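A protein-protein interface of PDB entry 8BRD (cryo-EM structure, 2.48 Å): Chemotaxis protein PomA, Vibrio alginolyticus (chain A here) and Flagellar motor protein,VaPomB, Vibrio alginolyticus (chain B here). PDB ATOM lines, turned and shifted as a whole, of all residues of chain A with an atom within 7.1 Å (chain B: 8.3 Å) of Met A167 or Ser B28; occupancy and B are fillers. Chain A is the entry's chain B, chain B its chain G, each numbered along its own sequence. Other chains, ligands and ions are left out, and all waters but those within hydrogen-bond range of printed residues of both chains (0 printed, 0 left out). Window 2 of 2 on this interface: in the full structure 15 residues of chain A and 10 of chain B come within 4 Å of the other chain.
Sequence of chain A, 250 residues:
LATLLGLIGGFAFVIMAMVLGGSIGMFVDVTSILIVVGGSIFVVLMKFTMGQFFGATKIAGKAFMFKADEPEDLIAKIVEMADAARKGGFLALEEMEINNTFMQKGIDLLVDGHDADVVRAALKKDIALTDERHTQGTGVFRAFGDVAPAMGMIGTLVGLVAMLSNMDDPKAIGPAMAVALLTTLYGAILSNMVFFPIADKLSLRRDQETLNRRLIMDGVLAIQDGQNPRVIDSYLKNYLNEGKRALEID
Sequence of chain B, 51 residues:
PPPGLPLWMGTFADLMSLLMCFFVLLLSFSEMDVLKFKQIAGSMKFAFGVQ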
ATOM      1  N   LEU A 160     -19.837 -14.174   6.479  1.00  0.00           N
ATOM      2  CA  LEU A 160     -20.739 -14.733   5.482  1.00  0.00           C
ATOM      3  C   LEU A 160     -21.804 -15.605   6.128  1.00  0.00           C
ATOM      4  O   LEU A 160     -22.960 -15.584   5.704  1.00  0.00           O
ATOM      5  CB  LEU A 160     -19.951 -15.515   4.434  1.00  0.00           C
ATOM      6  CG  LEU A 160     -19.086 -14.657   3.504  1.00  0.00           C
ATOM      7  CD1 LEU A 160     -18.454 -15.495   2.410  1.00  0.00           C
ATOM      8  CD2 LEU A 160     -19.881 -13.500   2.924  1.00  0.00           C
ATOM      9  N   ALA A 162     -22.963 -15.006   9.110  1.00  0.00           N
ATOM     10  CA  ALA A 162     -23.852 -14.005   9.686  1.00  0.00           C
ATOM     11  C   ALA A 162     -24.737 -13.349   8.633  1.00  0.00           C
ATOM     12  O   ALA A 162     -25.920 -13.111   8.889  1.00  0.00           O
ATOM     13  CB  ALA A 162     -23.041 -12.950  10.433  1.00  0.00           C
ATOM     14  N   MET A 163     -24.195 -13.053   7.454  1.00  0.00           N
ATOM     15  CA  MET A 163     -24.977 -12.392   6.416  1.00  0.00           C
ATOM     16  C   MET A 163     -26.037 -13.318   5.836  1.00  0.00           C
ATOM     17  O   MET A 163     -27.199 -12.929   5.693  1.00  0.00           O
ATOM     18  CB  MET A 163     -24.055 -11.882   5.308  1.00  0.00           C
ATOM     19  CG  MET A 163     -24.713 -10.891   4.364  1.00  0.00           C
ATOM     20  SD  MET A 163     -23.931 -10.830   2.741  1.00  0.00           S
ATOM     21  CE  MET A 163     -23.556 -12.560   2.466  1.00  0.00           C
ATOM     22  N   LEU A 164     -25.652 -14.550   5.501  1.00  0.00           N
ATOM     23  CA  LEU A 164     -26.593 -15.480   4.889  1.00  0.00           C
ATOM     24  C   LEU A 164     -27.653 -15.943   5.878  1.00  0.00           C
ATOM     25  O   LEU A 164     -28.745 -16.344   5.467  1.00  0.00           O
ATOM     26  CB  LEU A 164     -25.841 -16.675   4.313  1.00  0.00           C
ATOM     27  CG  LEU A 164     -24.716 -16.355   3.326  1.00  0.00           C
ATOM     28  CD1 LEU A 164     -23.777 -17.534   3.200  1.00  0.00           C
ATOM     29  CD2 LEU A 164     -25.259 -15.958   1.973  1.00  0.00           C
ATOM     30  N   SER A 165     -27.353 -15.897   7.177  1.00  0.00           N
ATOM     31  CA  SER A 165     -28.339 -16.312   8.167  1.00  0.00           C
ATOM     32  C   SER A 165     -29.418 -15.261   8.400  1.00  0.00           C
ATOM     33  O   SER A 165     -30.579 -15.618   8.622  1.00  0.00           O
ATOM     34  CB  SER A 165     -27.640 -16.646   9.478  1.00  0.00           C
ATOM     35  OG  SER A 165     -26.732 -17.717   9.304  1.00  0.00           O
ATOM     36  N   ASN A 166     -29.070 -13.977   8.353  1.00  0.00           N
ATOM     37  CA  ASN A 166     -30.008 -12.887   8.605  1.00  0.00           C
ATOM     38  C   ASN A 166     -30.341 -12.118   7.331  1.00  0.00           C
ATOM     39  O   ASN A 166     -30.367 -10.887   7.319  1.00  0.00           O
ATOM     40  CB  ASN A 166     -29.485 -11.932   9.677  1.00  0.00           C
ATOM     41  CG  ASN A 166     -28.609 -12.619  10.699  1.00  0.00           C
ATOM     42  OD1 ASN A 166     -27.441 -12.279  10.863  1.00  0.00           O
ATOM     43  ND2 ASN A 166     -29.174 -13.594  11.398  1.00  0.00           N
ATOM     44  N   MET A 167     -30.582 -12.846   6.241  1.00  0.00           N
ATOM     45  CA  MET A 167     -30.905 -12.206   4.969  1.00  0.00           C
ATOM     46  C   MET A 167     -32.145 -11.330   5.071  1.00  0.00           C
ATOM     47  O   MET A 167     -32.253 -10.323   4.362  1.00  0.00           O
ATOM     48  CB  MET A 167     -31.113 -13.264   3.891  1.00  0.00           C
ATOM     49  CG  MET A 167     -30.441 -12.937   2.586  1.00  0.00           C
ATOM     50  SD  MET A 167     -28.666 -13.195   2.633  1.00  0.00           S
ATOM     51  CE  MET A 167     -28.582 -14.759   1.776  1.00  0.00           C
ATOM     52  N   ASP A 168     -33.091 -11.691   5.934  1.00  0.00           N
ATOM     53  CA  ASP A 168     -34.305 -10.906   6.118  1.00  0.00           C
ATOM     54  C   ASP A 168     -34.095  -9.698   7.020  1.00  0.00           C
ATOM     55  O   ASP A 168     -35.041  -8.934   7.234  1.00  0.00           O
ATOM     56  CB  ASP A 168     -35.420 -11.786   6.684  1.00  0.00           C
ATOM     57  CG  ASP A 168     -35.698 -13.003   5.822  1.00  0.00           C
ATOM     58  OD1 ASP A 168     -35.311 -12.993   4.636  1.00  0.00           O
ATOM     59  OD2 ASP A 168     -36.306 -13.968   6.329  1.00  0.00           O
ATOM     60  N   ASP A 169     -32.889  -9.511   7.550  1.00  0.00           N
ATOM     61  CA  ASP A 169     -32.564  -8.374   8.411  1.00  0.00           C
ATOM     62  C   ASP A 169     -31.533  -7.509   7.699  1.00  0.00           C
ATOM     63  O   ASP A 169     -30.323  -7.784   7.790  1.00  0.00           O
ATOM     64  CB  ASP A 169     -32.026  -8.849   9.759  1.00  0.00           C
ATOM     65  CG  ASP A 169     -32.006  -7.749  10.796  1.00  0.00           C
ATOM     66  OD1 ASP A 169     -32.530  -6.655  10.507  1.00  0.00           O
ATOM     67  OD2 ASP A 169     -31.459  -7.974  11.896  1.00  0.00           O
ATOM     68  N   PRO A 170     -31.956  -6.473   6.972  1.00  0.00           N
ATOM     69  CA  PRO A 170     -30.976  -5.655   6.234  1.00  0.00           C
ATOM     70  C   PRO A 170     -29.917  -5.012   7.114  1.00  0.00           C
ATOM     71  O   PRO A 170     -28.745  -4.964   6.724  1.00  0.00           O
ATOM     72  CB  PRO A 170     -31.860  -4.612   5.536  1.00  0.00           C
ATOM     73  CG  PRO A 170     -33.183  -5.282   5.401  1.00  0.00           C
ATOM     74  CD  PRO A 170     -33.343  -6.103   6.644  1.00  0.00           C
ATOM     75  N   ALA A 172     -28.467  -6.110   9.616  1.00  0.00           N
ATOM     76  CA  ALA A 172     -27.441  -7.074   9.981  1.00  0.00           C
ATOM     77  C   ALA A 172     -26.608  -7.531   8.793  1.00  0.00           C
ATOM     78  O   ALA A 172     -25.504  -8.047   8.992  1.00  0.00           O
ATOM     79  CB  ALA A 172     -28.074  -8.300  10.651  1.00  0.00           C
ATOM     80  N   ILE A 173     -27.115  -7.353   7.571  1.00  0.00           N
ATOM     81  CA  ILE A 173     -26.386  -7.755   6.373  1.00  0.00           C
ATOM     82  C   ILE A 173     -25.141  -6.901   6.180  1.00  0.00           C
ATOM     83  O   ILE A 173     -24.059  -7.419   5.884  1.00  0.00           O
ATOM     84  CB  ILE A 173     -27.318  -7.681   5.150  1.00  0.00           C
ATOM     85  CG1 ILE A 173     -28.335  -8.820   5.186  1.00  0.00           C
ATOM     86  CG2 ILE A 173     -26.519  -7.718   3.861  1.00  0.00           C
ATOM     87  CD1 ILE A 173     -29.375  -8.731   4.103  1.00  0.00           C
ATOM     88  N   CYS B  21     -20.951 -15.323  -2.230  1.00  0.00           N
ATOM     89  CA  CYS B  21     -21.977 -15.073  -1.228  1.00  0.00           C
ATOM     90  C   CYS B  21     -22.645 -13.723  -1.440  1.00  0.00           C
ATOM     91  O   CYS B  21     -23.809 -13.545  -1.071  1.00  0.00           O
ATOM     92  CB  CYS B  21     -21.377 -15.186   0.168  1.00  0.00           C
ATOM     93  SG  CYS B  21     -21.221 -16.891   0.726  1.00  0.00           S
ATOM     94  N   PHE B  22     -21.946 -12.771  -2.061  1.00  0.00           N
ATOM     95  CA  PHE B  22     -22.608 -11.544  -2.492  1.00  0.00           C
ATOM     96  C   PHE B  22     -23.659 -11.836  -3.555  1.00  0.00           C
ATOM     97  O   PHE B  22     -24.740 -11.235  -3.556  1.00  0.00           O
ATOM     98  CB  PHE B  22     -21.578 -10.544  -3.013  1.00  0.00           C
ATOM     99  CG  PHE B  22     -22.160  -9.202  -3.350  1.00  0.00           C
ATOM    100  CD1 PHE B  22     -22.814  -8.457  -2.385  1.00  0.00           C
ATOM    101  CD2 PHE B  22     -22.065  -8.690  -4.629  1.00  0.00           C
ATOM    102  CE1 PHE B  22     -23.353  -7.232  -2.688  1.00  0.00           C
ATOM    103  CE2 PHE B  22     -22.604  -7.461  -4.937  1.00  0.00           C
ATOM    104  CZ  PHE B  22     -23.249  -6.732  -3.966  1.00  0.00           C
ATOM    105  N   PHE B  23     -23.360 -12.757  -4.469  1.00  0.00           N
ATOM    106  CA  PHE B  23     -24.350 -13.130  -5.475  1.00  0.00           C
ATOM    107  C   PHE B  23     -25.503 -13.906  -4.854  1.00  0.00           C
ATOM    108  O   PHE B  23     -26.645 -13.790  -5.302  1.00  0.00           O
ATOM    109  CB  PHE B  23     -23.692 -13.930  -6.596  1.00  0.00           C
ATOM    110  CG  PHE B  23     -22.728 -13.128  -7.404  1.00  0.00           C
ATOM    111  CD1 PHE B  23     -23.081 -11.880  -7.878  1.00  0.00           C
ATOM    112  CD2 PHE B  23     -21.464 -13.610  -7.679  1.00  0.00           C
ATOM    113  CE1 PHE B  23     -22.192 -11.129  -8.609  1.00  0.00           C
ATOM    114  CE2 PHE B  23     -20.570 -12.859  -8.405  1.00  0.00           C
ATOM    115  CZ  PHE B  23     -20.935 -11.620  -8.872  1.00  0.00           C
ATOM    116  N   VAL B  24     -25.226 -14.702  -3.819  1.00  0.00           N
ATOM    117  CA  VAL B  24     -26.309 -15.347  -3.076  1.00  0.00           C
ATOM    118  C   VAL B  24     -27.194 -14.304  -2.402  1.00  0.00           C
ATOM    119  O   VAL B  24     -28.427 -14.423  -2.402  1.00  0.00           O
ATOM    120  CB  VAL B  24     -25.747 -16.357  -2.056  1.00  0.00           C
ATOM    121  CG1 VAL B  24     -26.878 -17.029  -1.300  1.00  0.00           C
ATOM    122  CG2 VAL B  24     -24.911 -17.399  -2.759  1.00  0.00           C
ATOM    123  N   LEU B  25     -26.584 -13.265  -1.830  1.00  0.00           N
ATOM    124  CA  LEU B  25     -27.351 -12.166  -1.255  1.00  0.00           C
ATOM    125  C   LEU B  25     -28.220 -11.490  -2.309  1.00  0.00           C
ATOM    126  O   LEU B  25     -29.389 -11.184  -2.058  1.00  0.00           O
ATOM    127  CB  LEU B  25     -26.410 -11.151  -0.610  1.00  0.00           C
ATOM    128  CG  LEU B  25     -27.055  -9.856  -0.109  1.00  0.00           C
ATOM    129  CD1 LEU B  25     -27.959 -10.121   1.071  1.00  0.00           C
ATOM    130  CD2 LEU B  25     -25.996  -8.833   0.243  1.00  0.00           C
ATOM    131  N   LEU B  26     -27.661 -11.243  -3.495  1.00  0.00           N
ATOM    132  CA  LEU B  26     -28.442 -10.624  -4.562  1.00  0.00           C
ATOM    133  C   LEU B  26     -29.567 -11.532  -5.039  1.00  0.00           C
ATOM    134  O   LEU B  26     -30.646 -11.048  -5.391  1.00  0.00           O
ATOM    135  CB  LEU B  26     -27.538 -10.246  -5.734  1.00  0.00           C
ATOM    136  CG  LEU B  26     -26.499  -9.160  -5.459  1.00  0.00           C
ATOM    137  CD1 LEU B  26     -25.818  -8.738  -6.744  1.00  0.00           C
ATOM    138  CD2 LEU B  26     -27.159  -7.967  -4.788  1.00  0.00           C
ATOM    139  N   LEU B  27     -29.335 -12.843  -5.054  1.00  0.00           N
ATOM    140  CA  LEU B  27     -30.362 -13.786  -5.463  1.00  0.00           C
ATOM    141  C   LEU B  27     -31.419 -13.987  -4.389  1.00  0.00           C
ATOM    142  O   LEU B  27     -32.487 -14.530  -4.686  1.00  0.00           O
ATOM    143  CB  LEU B  27     -29.719 -15.128  -5.813  1.00  0.00           C
ATOM    144  CG  LEU B  27     -29.298 -15.322  -7.265  1.00  0.00           C
ATOM    145  CD1 LEU B  27     -28.386 -16.520  -7.391  1.00  0.00           C
ATOM    146  CD2 LEU B  27     -30.518 -15.483  -8.149  1.00  0.00           C
ATOM    147  N   SER B  28     -31.144 -13.567  -3.153  1.00  0.00           N
ATOM    148  CA  SER B  28     -32.125 -13.738  -2.086  1.00  0.00           C
ATOM    149  C   SER B  28     -33.358 -12.872  -2.303  1.00  0.00           C
ATOM    150  O   SER B  28     -34.469 -13.283  -1.953  1.00  0.00           O
ATOM    151  CB  SER B  28     -31.494 -13.412  -0.737  1.00  0.00           C
ATOM    152  OG  SER B  28     -31.232 -12.027  -0.625  1.00  0.00           O
ATOM    153  N   PHE B  29     -33.192 -11.683  -2.878  1.00  0.00           N
ATOM    154  CA  PHE B  29     -34.298 -10.756  -3.078  1.00  0.00           C
ATOM    155  C   PHE B  29     -34.569 -10.524  -4.560  1.00  0.00           C
ATOM    156  O   PHE B  29     -35.049  -9.462  -4.955  1.00  0.00           O
ATOM    157  CB  PHE B  29     -34.033  -9.431  -2.361  1.00  0.00           C
ATOM    158  CG  PHE B  29     -32.798  -8.717  -2.831  1.00  0.00           C
ATOM    159  CD1 PHE B  29     -31.572  -8.977  -2.251  1.00  0.00           C
ATOM    160  CD2 PHE B  29     -32.864  -7.779  -3.846  1.00  0.00           C
ATOM    161  CE1 PHE B  29     -30.437  -8.323  -2.683  1.00  0.00           C
ATOM    162  CE2 PHE B  29     -31.734  -7.124  -4.278  1.00  0.00           C
ATOM    163  CZ  PHE B  29     -30.519  -7.397  -3.693  1.00  0.00           C
ATOM    164  N   SER B  30     -34.286 -11.524  -5.388  1.00  0.00           N
ATOM    165  CA  SER B  30     -34.437 -11.419  -6.832  1.00  0.00           C
ATOM    166  C   SER B  30     -35.416 -12.483  -7.299  1.00  0.00           C
ATOM    167  O   SER B  30     -35.229 -13.671  -7.014  1.00  0.00           O
ATOM    168  CB  SER B  30     -33.093 -11.585  -7.539  1.00  0.00           C
ATOM    169  OG  SER B  30     -32.849 -12.948  -7.819  1.00  0.00           O
ATOM    170  N   GLU B  31     -36.452 -12.059  -8.013  1.00  0.00           N
ATOM    171  CA  GLU B  31     -37.436 -12.982  -8.553  1.00  0.00           C
ATOM    172  C   GLU B  31     -37.047 -13.394  -9.964  1.00  0.00           C
ATOM    173  O   GLU B  31     -36.560 -12.582 -10.754  1.00  0.00           O
ATOM    174  CB  GLU B  31     -38.831 -12.354  -8.552  1.00  0.00           C
ATOM    175  CG  GLU B  31     -39.947 -13.367  -8.378  1.00  0.00           C
ATOM    176  CD  GLU B  31     -40.122 -13.790  -6.933  1.00  0.00           C
ATOM    177  OE1 GLU B  31     -39.568 -13.112  -6.041  1.00  0.00           O
ATOM    178  OE2 GLU B  31     -40.810 -14.803  -6.691  1.00  0.00           O
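Along chain A the printed residues that touch a printed residue of chain B span positions 160 to 173. Hydrophobic or aromatic side chains of chain B that line the printed part of chain A: Val B24 and Leu B25.
Met A167 touches two residues of chain B. Of the printed residues of chain A, Ser B28 touches Met A167. Of the printed residues of chain B, Ile A173 touches Leu B25. Of the printed residues of chain B, Leu A160 touches Cys B21. Of the printed residues of chain B, Met A163 touches Cys B21 and Leu B25. Of the printed residues of chain A, Leu B25 touches Met A163, Met A167 and Ile A173. Ser B30 touches none of the printed residues of chain A. Phe B22 touches none of the printed residues of chain A. The nearest residue of chain B that does not touch Met A167 is Val B24 (4.2 Å). The nearest printed residue of chain B that does not touch Ile A173 is Ser B28 (6.1 Å).
Among the printed residues, pairs that only touch across the chains: Leu A160 with Cys B21, Met A163 with Cys B21, Met A163 with Leu B25, Leu A164 with Cys B21, Leu A164 with Val B24, Met A167 with Leu B25, Met A167 with Ser B28 and Ile A173 with Leu B25.
OG of Ser B28 sits at hydrogen-bond distance from O of Leu B25, 2.5 Å away.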
